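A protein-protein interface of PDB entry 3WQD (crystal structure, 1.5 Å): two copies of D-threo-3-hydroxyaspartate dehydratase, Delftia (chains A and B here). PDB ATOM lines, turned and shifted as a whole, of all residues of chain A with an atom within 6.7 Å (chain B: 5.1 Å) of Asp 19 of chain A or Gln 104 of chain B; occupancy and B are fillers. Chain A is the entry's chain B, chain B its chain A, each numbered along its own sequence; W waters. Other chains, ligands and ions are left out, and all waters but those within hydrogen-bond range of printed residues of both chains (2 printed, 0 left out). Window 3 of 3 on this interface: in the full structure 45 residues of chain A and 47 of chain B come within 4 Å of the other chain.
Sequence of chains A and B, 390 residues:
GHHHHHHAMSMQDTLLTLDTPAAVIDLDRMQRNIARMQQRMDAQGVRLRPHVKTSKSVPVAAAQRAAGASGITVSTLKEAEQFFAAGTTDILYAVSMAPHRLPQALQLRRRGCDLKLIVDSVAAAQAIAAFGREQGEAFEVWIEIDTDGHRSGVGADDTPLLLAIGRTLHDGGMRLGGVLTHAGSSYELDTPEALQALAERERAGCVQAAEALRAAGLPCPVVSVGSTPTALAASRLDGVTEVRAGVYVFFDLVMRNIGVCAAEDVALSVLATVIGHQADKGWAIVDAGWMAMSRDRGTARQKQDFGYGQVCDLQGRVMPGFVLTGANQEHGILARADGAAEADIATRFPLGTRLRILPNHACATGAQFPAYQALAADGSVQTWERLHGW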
ATOM      1  N   ASP A  13       5.739  18.676  18.279  1.00  0.00           N
ATOM      2  CA  ASP A  13       5.147  17.993  17.105  1.00  0.00           C
ATOM      3  C   ASP A  13       4.023  17.047  17.417  1.00  0.00           C
ATOM      4  O   ASP A  13       3.893  16.554  18.567  1.00  0.00           O
ATOM      5  CB  ASP A  13       6.224  17.282  16.258  1.00  0.00           C
ATOM      6  CG  ASP A  13       6.998  18.261  15.374  1.00  0.00           C
ATOM      7  OD1 ASP A  13       6.427  18.960  14.524  1.00  0.00           O
ATOM      8  OD2 ASP A  13       8.192  18.372  15.551  1.00  0.00           O
ATOM      9  N   THR A  14       3.194  16.775  16.417  1.00  0.00           N
ATOM     10  CA  THR A  14       2.113  15.798  16.550  1.00  0.00           C
ATOM     11  C   THR A  14       2.167  14.990  15.260  1.00  0.00           C
ATOM     12  O   THR A  14       3.023  15.270  14.375  1.00  0.00           O
ATOM     13  CB  THR A  14       0.761  16.524  16.580  1.00  0.00           C
ATOM     14  OG1 THR A  14       0.579  17.090  15.282  1.00  0.00           O
ATOM     15  CG2 THR A  14       0.689  17.665  17.664  1.00  0.00           C
ATOM     16  N   LEU A  16       0.298  15.290  12.831  1.00  0.00           N
ATOM     17  CA  LEU A  16      -0.014  16.156  11.685  1.00  0.00           C
ATOM     18  C   LEU A  16       1.139  17.010  11.236  1.00  0.00           C
ATOM     19  O   LEU A  16       1.112  17.542  10.099  1.00  0.00           O
ATOM     20  CB  LEU A  16      -1.192  17.091  12.062  1.00  0.00           C
ATOM     21  CG  LEU A  16      -2.557  16.383  12.176  1.00  0.00           C
ATOM     22  CD1 LEU A  16      -3.613  17.361  12.723  1.00  0.00           C
ATOM     23  CD2 LEU A  16      -2.990  15.831  10.795  1.00  0.00           C
ATOM     24  N   THR A  17       2.113  17.235  12.130  1.00  0.00           N
ATOM     25  CA  THR A  17       3.182  18.180  11.831  1.00  0.00           C
ATOM     26  C   THR A  17       4.499  17.481  11.504  1.00  0.00           C
ATOM     27  O   THR A  17       5.370  18.114  10.935  1.00  0.00           O
ATOM     28  CB  THR A  17       3.472  19.182  12.980  1.00  0.00           C
ATOM     29  OG1 THR A  17       3.916  18.457  14.139  1.00  0.00           O
ATOM     30  CG2 THR A  17       2.204  20.002  13.348  1.00  0.00           C
ATOM     31  N   LEU A  18       4.659  16.195  11.837  1.00  0.00           N
ATOM     32  CA  LEU A  18       5.902  15.471  11.478  1.00  0.00           C
ATOM     33  C   LEU A  18       6.058  15.412   9.949  1.00  0.00           C
ATOM     34  O   LEU A  18       5.054  15.245   9.217  1.00  0.00           O
ATOM     35  CB  LEU A  18       5.809  14.017  12.018  1.00  0.00           C
ATOM     36  CG  LEU A  18       6.022  13.867  13.530  1.00  0.00           C
ATOM     37  CD1 LEU A  18       5.744  12.411  13.853  1.00  0.00           C
ATOM     38  CD2 LEU A  18       7.450  14.284  13.963  1.00  0.00           C
ATOM     39  N   ASP A  19       7.299  15.428   9.475  1.00  0.00           N
ATOM     40  CA  ASP A  19       7.531  15.000   8.111  1.00  0.00           C
ATOM     41  C   ASP A  19       7.378  13.469   8.046  1.00  0.00           C
ATOM     42  O   ASP A  19       7.455  12.759   9.075  1.00  0.00           O
ATOM     43  CB  ASP A  19       8.947  15.394   7.657  1.00  0.00           C
ATOM     44  CG  ASP A  19       9.155  15.297   6.111  1.00  0.00           C
ATOM     45  OD1 ASP A  19       8.122  15.278   5.348  1.00  0.00           O
ATOM     46  OD2 ASP A  19      10.350  15.163   5.647  1.00  0.00           O
ATOM     47  N   THR A  20       7.060  12.987   6.850  1.00  0.00           N
ATOM     48  CA  THR A  20       6.862  11.559   6.611  1.00  0.00           C
ATOM     49  C   THR A  20       7.929  11.114   5.617  1.00  0.00           C
ATOM     50  O   THR A  20       8.437  11.918   4.774  1.00  0.00           O
ATOM     51  CB  THR A  20       5.454  11.294   6.040  1.00  0.00           C
ATOM     52  OG1 THR A  20       5.249  12.139   4.884  1.00  0.00           O
ATOM     53  CG2 THR A  20       4.407  11.604   7.105  1.00  0.00           C
ATOM     54  N   PRO A  21       8.350   9.857   5.689  1.00  0.00           N
ATOM     55  CA  PRO A  21       7.860   8.849   6.630  1.00  0.00           C
ATOM     56  C   PRO A  21       8.494   9.030   8.030  1.00  0.00           C
ATOM     57  O   PRO A  21       9.603   9.543   8.151  1.00  0.00           O
ATOM     58  CB  PRO A  21       8.322   7.528   5.987  1.00  0.00           C
ATOM     59  CG  PRO A  21       9.616   7.907   5.281  1.00  0.00           C
ATOM     60  CD  PRO A  21       9.370   9.353   4.725  1.00  0.00           C
ATOM     61  N   ALA A  22       7.803   8.482   9.037  1.00  0.00           N
ATOM     62  CA  ALA A  22       8.316   8.524  10.412  1.00  0.00           C
ATOM     63  C   ALA A  22       7.915   7.231  11.111  1.00  0.00           C
ATOM     64  O   ALA A  22       6.826   6.680  10.846  1.00  0.00           O
ATOM     65  CB  ALA A  22       7.654   9.696  11.158  1.00  0.00           C
ATOM     66  N   LEU A 271       4.303   6.308   9.704  1.00  0.00           N
ATOM     67  CA  LEU A 271       3.437   7.446   9.281  1.00  0.00           C
ATOM     68  C   LEU A 271       3.843   7.790   7.845  1.00  0.00           C
ATOM     69  O   LEU A 271       5.025   7.955   7.592  1.00  0.00           O
ATOM     70  CB  LEU A 271       3.708   8.636  10.196  1.00  0.00           C
ATOM     71  CG  LEU A 271       2.788   9.843   9.993  1.00  0.00           C
ATOM     72  CD1 LEU A 271       1.332   9.522  10.436  1.00  0.00           C
ATOM     73  CD2 LEU A 271       3.385  11.024  10.743  1.00  0.00           C
ATOM     74  N   THR A 273       2.608   9.705   3.844  1.00  0.00           N
ATOM     75  CA  THR A 273       1.706  10.603   3.145  1.00  0.00           C
ATOM     76  C   THR A 273       1.380  10.062   1.751  1.00  0.00           C
ATOM     77  O   THR A 273       2.305   9.579   1.058  1.00  0.00           O
ATOM     78  CB  THR A 273       2.392  12.042   2.984  1.00  0.00           C
ATOM     79  OG1 THR A 273       2.591  12.573   4.297  1.00  0.00           O
ATOM     80  CG2 THR A 273       1.469  13.046   2.234  1.00  0.00           C
ATOM     81  N   ASP A 287       4.698   7.921   0.349  1.00  0.00           N
ATOM     82  CA  ASP A 287       6.157   8.206   0.513  1.00  0.00           C
ATOM     83  C   ASP A 287       6.862   7.252   1.476  1.00  0.00           C
ATOM     84  O   ASP A 287       7.987   7.527   1.895  1.00  0.00           O
ATOM     85  CB  ASP A 287       6.402   9.689   0.859  1.00  0.00           C
ATOM     86  CG  ASP A 287       5.850  10.076   2.220  1.00  0.00           C
ATOM     87  OD1 ASP A 287       5.230   9.247   2.935  1.00  0.00           O
ATOM     88  OD2 ASP A 287       5.976  11.256   2.616  1.00  0.00           O
ATOM     89  N   ARG A 354      -2.679  11.390   5.440  1.00  0.00           N
ATOM     90  CA  ARG A 354      -1.651  10.661   6.211  1.00  0.00           C
ATOM     91  C   ARG A 354      -2.236   9.344   6.656  1.00  0.00           C
ATOM     92  O   ARG A 354      -3.403   9.280   7.117  1.00  0.00           O
ATOM     93  CB  ARG A 354      -1.195  11.465   7.433  1.00  0.00           C
ATOM     94  CG  ARG A 354      -0.463  12.731   7.032  1.00  0.00           C
ATOM     95  CD  ARG A 354      -0.052  13.626   8.171  1.00  0.00           C
ATOM     96  NE  ARG A 354       0.871  14.583   7.540  1.00  0.00           N
ATOM     97  CZ  ARG A 354       2.084  14.884   7.992  1.00  0.00           C
ATOM     98  NH1 ARG A 354       2.438  14.515   9.209  1.00  0.00           N
ATOM     99  NH2 ARG A 354       2.875  15.682   7.279  1.00  0.00           N
ATOM    100  N   GLN A 373       9.400   8.320  16.848  1.00  0.00           N
ATOM    101  CA  GLN A 373       8.566   9.425  17.373  1.00  0.00           C
ATOM    102  C   GLN A 373       7.668   8.717  18.389  1.00  0.00           C
ATOM    103  O   GLN A 373       6.751   7.973  17.974  1.00  0.00           O
ATOM    104  CB  GLN A 373       7.770  10.037  16.204  1.00  0.00           C
ATOM    105  CG  GLN A 373       8.736  10.850  15.316  1.00  0.00           C
ATOM    106  CD  GLN A 373       9.456  12.000  16.091  1.00  0.00           C
ATOM    107  OE1 GLN A 373       8.893  12.562  17.013  1.00  0.00           O
ATOM    108  NE2 GLN A 373      10.661  12.305  15.755  1.00  0.00           N
ATOM    109  N   LEU B  77      14.450  15.104   0.377  1.00  0.00           N
ATOM    110  CA  LEU B  77      15.010  16.467   0.648  1.00  0.00           C
ATOM    111  C   LEU B  77      16.179  16.432   1.632  1.00  0.00           C
ATOM    112  O   LEU B  77      17.027  17.312   1.562  1.00  0.00           O
ATOM    113  CB  LEU B  77      13.945  17.444   1.148  1.00  0.00           C
ATOM    114  CG  LEU B  77      12.924  17.705   0.032  1.00  0.00           C
ATOM    115  CD1 LEU B  77      11.936  18.792   0.585  1.00  0.00           C
ATOM    116  CD2 LEU B  77      13.619  18.307  -1.202  1.00  0.00           C
ATOM    117  N   GLU B  81      19.510  18.525   1.126  1.00  0.00           N
ATOM    118  CA  GLU B  81      20.205  19.312   2.148  1.00  0.00           C
ATOM    119  C   GLU B  81      21.717  18.945   2.246  1.00  0.00           C
ATOM    120  O   GLU B  81      22.599  19.847   2.303  1.00  0.00           O
ATOM    121  CB  GLU B  81      19.601  19.148   3.540  1.00  0.00           C
ATOM    122  CG  GLU B  81      18.161  19.544   3.626  1.00  0.00           C
ATOM    123  CD  GLU B  81      17.965  21.016   3.904  1.00  0.00           C
ATOM    124  OE1 GLU B  81      16.779  21.464   4.029  1.00  0.00           O
ATOM    125  OE2 GLU B  81      19.036  21.703   4.081  1.00  0.00           O
ATOM    126  N   HIS B 100       3.059  19.258   1.719  1.00  0.00           N
ATOM    127  CA  HIS B 100       3.535  19.615   3.059  1.00  0.00           C
ATOM    128  C   HIS B 100       5.053  19.878   3.082  1.00  0.00           C
ATOM    129  O   HIS B 100       5.522  20.508   4.035  1.00  0.00           O
ATOM    130  CB  HIS B 100       3.067  18.620   4.116  1.00  0.00           C
ATOM    131  CG  HIS B 100       3.885  17.396   4.189  1.00  0.00           C
ATOM    132  ND1 HIS B 100       3.550  16.250   3.507  1.00  0.00           N
ATOM    133  CD2 HIS B 100       5.065  17.136   4.860  1.00  0.00           C
ATOM    134  CE1 HIS B 100       4.477  15.294   3.746  1.00  0.00           C
ATOM    135  NE2 HIS B 100       5.417  15.823   4.570  1.00  0.00           N
ATOM    136  N   ARG B 101       5.822  19.346   2.116  1.00  0.00           N
ATOM    137  CA  ARG B 101       7.259  19.641   2.066  1.00  0.00           C
ATOM    138  C   ARG B 101       7.610  20.936   1.311  1.00  0.00           C
ATOM    139  O   ARG B 101       8.794  21.285   1.188  1.00  0.00           O
ATOM    140  CB  ARG B 101       7.978  18.455   1.393  1.00  0.00           C
ATOM    141  CG  ARG B 101       8.135  17.264   2.354  1.00  0.00           C
ATOM    142  CD  ARG B 101       9.035  16.173   1.738  1.00  0.00           C
ATOM    143  NE  ARG B 101       8.277  15.138   0.998  1.00  0.00           N
ATOM    144  CZ  ARG B 101       7.709  14.062   1.553  1.00  0.00           C
ATOM    145  NH1 ARG B 101       7.639  13.900   2.867  1.00  0.00           N
ATOM    146  NH2 ARG B 101       7.095  13.186   0.771  1.00  0.00           N
ATOM    147  N   LEU B 102       6.591  21.703   0.887  1.00  0.00           N
ATOM    148  CA  LEU B 102       6.884  22.932   0.128  1.00  0.00           C
ATOM    149  C   LEU B 102       7.714  23.946   0.967  1.00  0.00           C
ATOM    150  O   LEU B 102       8.608  24.569   0.414  1.00  0.00           O
ATOM    151  CB  LEU B 102       5.615  23.528  -0.465  1.00  0.00           C
ATOM    152  CG  LEU B 102       5.235  22.848  -1.811  1.00  0.00           C
ATOM    153  CD1 LEU B 102       3.768  23.184  -2.119  1.00  0.00           C
ATOM    154  CD2 LEU B 102       6.148  23.303  -2.970  1.00  0.00           C
ATOM    155  N   PRO B 103       7.392  24.144   2.283  1.00  0.00           N
ATOM    156  CA  PRO B 103       8.302  25.055   3.041  1.00  0.00           C
ATOM    157  C   PRO B 103       9.766  24.688   3.032  1.00  0.00           C
ATOM    158  O   PRO B 103      10.623  25.581   2.902  1.00  0.00           O
ATOM    159  CB  PRO B 103       7.689  25.104   4.449  1.00  0.00           C
ATOM    160  CG  PRO B 103       6.216  24.776   4.212  1.00  0.00           C
ATOM    161  CD  PRO B 103       6.213  23.752   3.094  1.00  0.00           C
ATOM    162  N   GLN B 104      10.072  23.378   3.087  1.00  0.00           N
ATOM    163  CA  GLN B 104      11.441  22.834   3.056  1.00  0.00           C
ATOM    164  C   GLN B 104      12.064  23.157   1.691  1.00  0.00           C
ATOM    165  O   GLN B 104      13.211  23.607   1.554  1.00  0.00           O
ATOM    166  CB  GLN B 104      11.349  21.279   3.279  1.00  0.00           C
ATOM    167  CG  GLN B 104      11.034  20.795   4.726  1.00  0.00           C
ATOM    168  CD  GLN B 104      10.570  19.307   4.865  1.00  0.00           C
ATOM    169  OE1 GLN B 104      11.298  18.392   4.522  1.00  0.00           O
ATOM    170  NE2 GLN B 104       9.377  19.085   5.425  1.00  0.00           N
ATOM    171  N   ALA B 105      11.289  22.901   0.615  1.00  0.00           N
ATOM    172  CA  ALA B 105      11.797  23.149  -0.728  1.00  0.00           C
ATOM    173  C   ALA B 105      12.043  24.639  -0.897  1.00  0.00           C
ATOM    174  O   ALA B 105      13.027  25.026  -1.591  1.00  0.00           O
ATOM    175  CB  ALA B 105      10.773  22.633  -1.763  1.00  0.00           C
ATOM    176  N   LEU B 106      11.111  25.473  -0.440  1.00  0.00           N
ATOM    177  CA  LEU B 106      11.304  26.933  -0.574  1.00  0.00           C
ATOM    178  C   LEU B 106      12.590  27.411   0.113  1.00  0.00           C
ATOM    179  O   LEU B 106      13.312  28.228  -0.464  1.00  0.00           O
ATOM    180  CB  LEU B 106      10.038  27.633   0.029  1.00  0.00           C
ATOM    181  CG  LEU B 106      10.102  29.187   0.082  1.00  0.00           C
ATOM    182  CD1 LEU B 106      10.182  29.690  -1.367  1.00  0.00           C
ATOM    183  CD2 LEU B 106       8.836  29.674   0.765  1.00  0.00           C
ATOM    184  N   GLN B 107      12.813  26.933   1.336  1.00  0.00           N
ATOM    185  CA  GLN B 107      13.958  27.373   2.085  1.00  0.00           C
ATOM    186  C   GLN B 107      15.264  26.959   1.346  1.00  0.00           C
ATOM    187  O   GLN B 107      16.189  27.751   1.256  1.00  0.00           O
ATOM    188  CB  GLN B 107      13.896  26.861   3.515  1.00  0.00           C
ATOM    189  CG  GLN B 107      14.975  27.486   4.325  1.00  0.00           C
ATOM    190  CD  GLN B 107      15.698  26.572   5.223  1.00  0.00           C
ATOM    191  OE1 GLN B 107      16.237  25.575   4.766  1.00  0.00           O
ATOM    192  NE2 GLN B 107      15.802  26.951   6.491  1.00  0.00           N
ATOM    193  N   LEU B 108      15.311  25.750   0.774  1.00  0.00           N
ATOM    194  CA  LEU B 108      16.422  25.356  -0.056  1.00  0.00           C
ATOM    195  C   LEU B 108      16.650  26.320  -1.193  1.00  0.00           C
ATOM    196  O   LEU B 108      17.810  26.705  -1.469  1.00  0.00           O
ATOM    197  CB  LEU B 108      16.322  23.899  -0.510  1.00  0.00           C
ATOM    198  CG  LEU B 108      16.787  22.890   0.531  1.00  0.00           C
ATOM    199  CD1 LEU B 108      16.134  21.512   0.184  1.00  0.00           C
ATOM    200  CD2 LEU B 108      18.349  22.846   0.568  1.00  0.00           C
ATOM    201  N   TRP B 390      15.540  10.736   6.966  1.00  0.00           N
ATOM    202  CA  TRP B 390      14.794  11.773   6.239  1.00  0.00           C
ATOM    203  C   TRP B 390      14.926  13.078   6.908  1.00  0.00           C
ATOM    204  O   TRP B 390      15.389  13.189   8.069  1.00  0.00           O
ATOM    205  CB  TRP B 390      13.287  11.357   6.148  1.00  0.00           C
ATOM    206  CG  TRP B 390      13.073  10.098   5.341  1.00  0.00           C
ATOM    207  CD1 TRP B 390      12.775   9.998   4.031  1.00  0.00           C
ATOM    208  CD2 TRP B 390      13.238   8.734   5.822  1.00  0.00           C
ATOM    209  NE1 TRP B 390      12.745   8.700   3.602  1.00  0.00           N
ATOM    210  CE2 TRP B 390      13.010   7.869   4.664  1.00  0.00           C
ATOM    211  CE3 TRP B 390      13.526   8.154   7.081  1.00  0.00           C
ATOM    212  CZ2 TRP B 390      13.048   6.460   4.767  1.00  0.00           C
ATOM    213  CZ3 TRP B 390      13.630   6.759   7.142  1.00  0.00           C
ATOM    214  CH2 TRP B 390      13.406   5.923   6.026  1.00  0.00           C
ATOM    215  OXT TRP B 390      14.508  14.071   6.282  1.00  0.00           O
HETATM  216  O   HOH W   1      12.303  15.259   7.412  1.00  0.00           O
HETATM  217  O   HOH W   2      10.100  11.654   2.352  1.00  0.00           O
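Water W1 lies within hydrogen-bond range of OD2 of Asp 19 of chain A and OXT of Trp 390 of chain B. Water W2 bridges the backbone carbonyl oxygen of Thr 20 of chain A (2.9 Å) and the guanidinium group of Arg 101 of chain B (3.4 Å).
Hydrophobic or aromatic side chains of chain B that line the printed part of chain A: His 100 and Trp 390. Of the 14 printed residues of chain A, 6 touch a printed residue of chain B. Among the printed residues, 9 pairs touch across the chains. Among the printed residues, Asp or Glu carboxylates within 4 Å of a Lys or Arg side-chain nitrogen of the other chain: Asp 19 of chain A with Arg 101 of chain B (2.9 Å) and Asp 287 of chain A with Arg 101 of chain B (2.9 Å).
Printed residues of chain B within 4 Å of Asp 19 of chain A: His 100 (2.9 Å), Arg 101 (2.9 Å) and Gln 104 (3.5 Å). Of the printed residues of chain A, Gln 104 of chain B touches Asp 19 (3.5 Å). Printed residues of chain A within 4 Å of His 100 of chain B: Asp 19 (2.9 Å), Thr 20 (3.4 Å), Thr 273 (3.4 Å) and Arg 354 (3.6 Å). Printed residues of chain A within 4 Å of Arg 101 of chain B: Asp 19, Thr 20 and Asp 287. Leu 16 of chain A touches none of the printed residues of chain B.
OG1 of Thr 20 of chain A sits at hydrogen-bond distance from OG1 of Thr 273 of chain A (2.8 Å). OD1 of Asp 287 of chain A sits at hydrogen-bond distance from N of Thr 273 of chain A (2.8 Å). The guanidinium group of Arg 354 of chain A sits at hydrogen-bond distance from the backbone carbonyl oxygen of Leu 16 of chain A (3.4 Å). A ring nitrogen (NE2) of His 100 of chain B is in hydrogen-bond range of the guanidinium group (NH1) of Arg 101 of chain B. The backbone carbonyl oxygen of Leu 18 of chain A sits at hydrogen-bond distance from the guanidinium group of Arg 354 of chain A (2.7 Å). OG1 of Thr 20 of chain A sits at hydrogen-bond distance from OD2 of Asp 287 of chain A (2.5 Å).
NH2 of Arg 101 of chain B lies within salt-bridge range of OD2 of Asp 287 of chain A, 2.9 Å away. A ring nitrogen (NE2) of His 100 of chain B is in hydrogen-bond range of the side-chain carboxylate (OD1) of Asp 19 of chain A (2.9 Å). The side-chain carboxylate (OD1) of Asp 19 of chain A lies within salt-bridge range of the guanidinium group (NH1) of Arg 101 of chain B (2.9 Å). The guanidinium group (NH1) of Arg 101 of chain B lies within hydrogen-bond range of the backbone carbonyl oxygen (O) of Thr 20 of chain A (2.9 Å).
No position is printed for both chains. Of the 9 pairs that touch across the chains among the printed residues, none has its exchanged pair printed and touching as well.
Among the printed residues, pairs that only touch across the chains: Thr 273 of chain A with His 100 of chain B (3.4 Å), Thr 20 of chain A with His 100 of chain B (3.4 Å), Pro 21 of chain A with Trp 390 of chain B (3.4 Å), Asp 19 of chain A with Gln 104 of chain B (3.5 Å) and Arg 354 of chain A with His 100 of chain B (3.6 Å).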
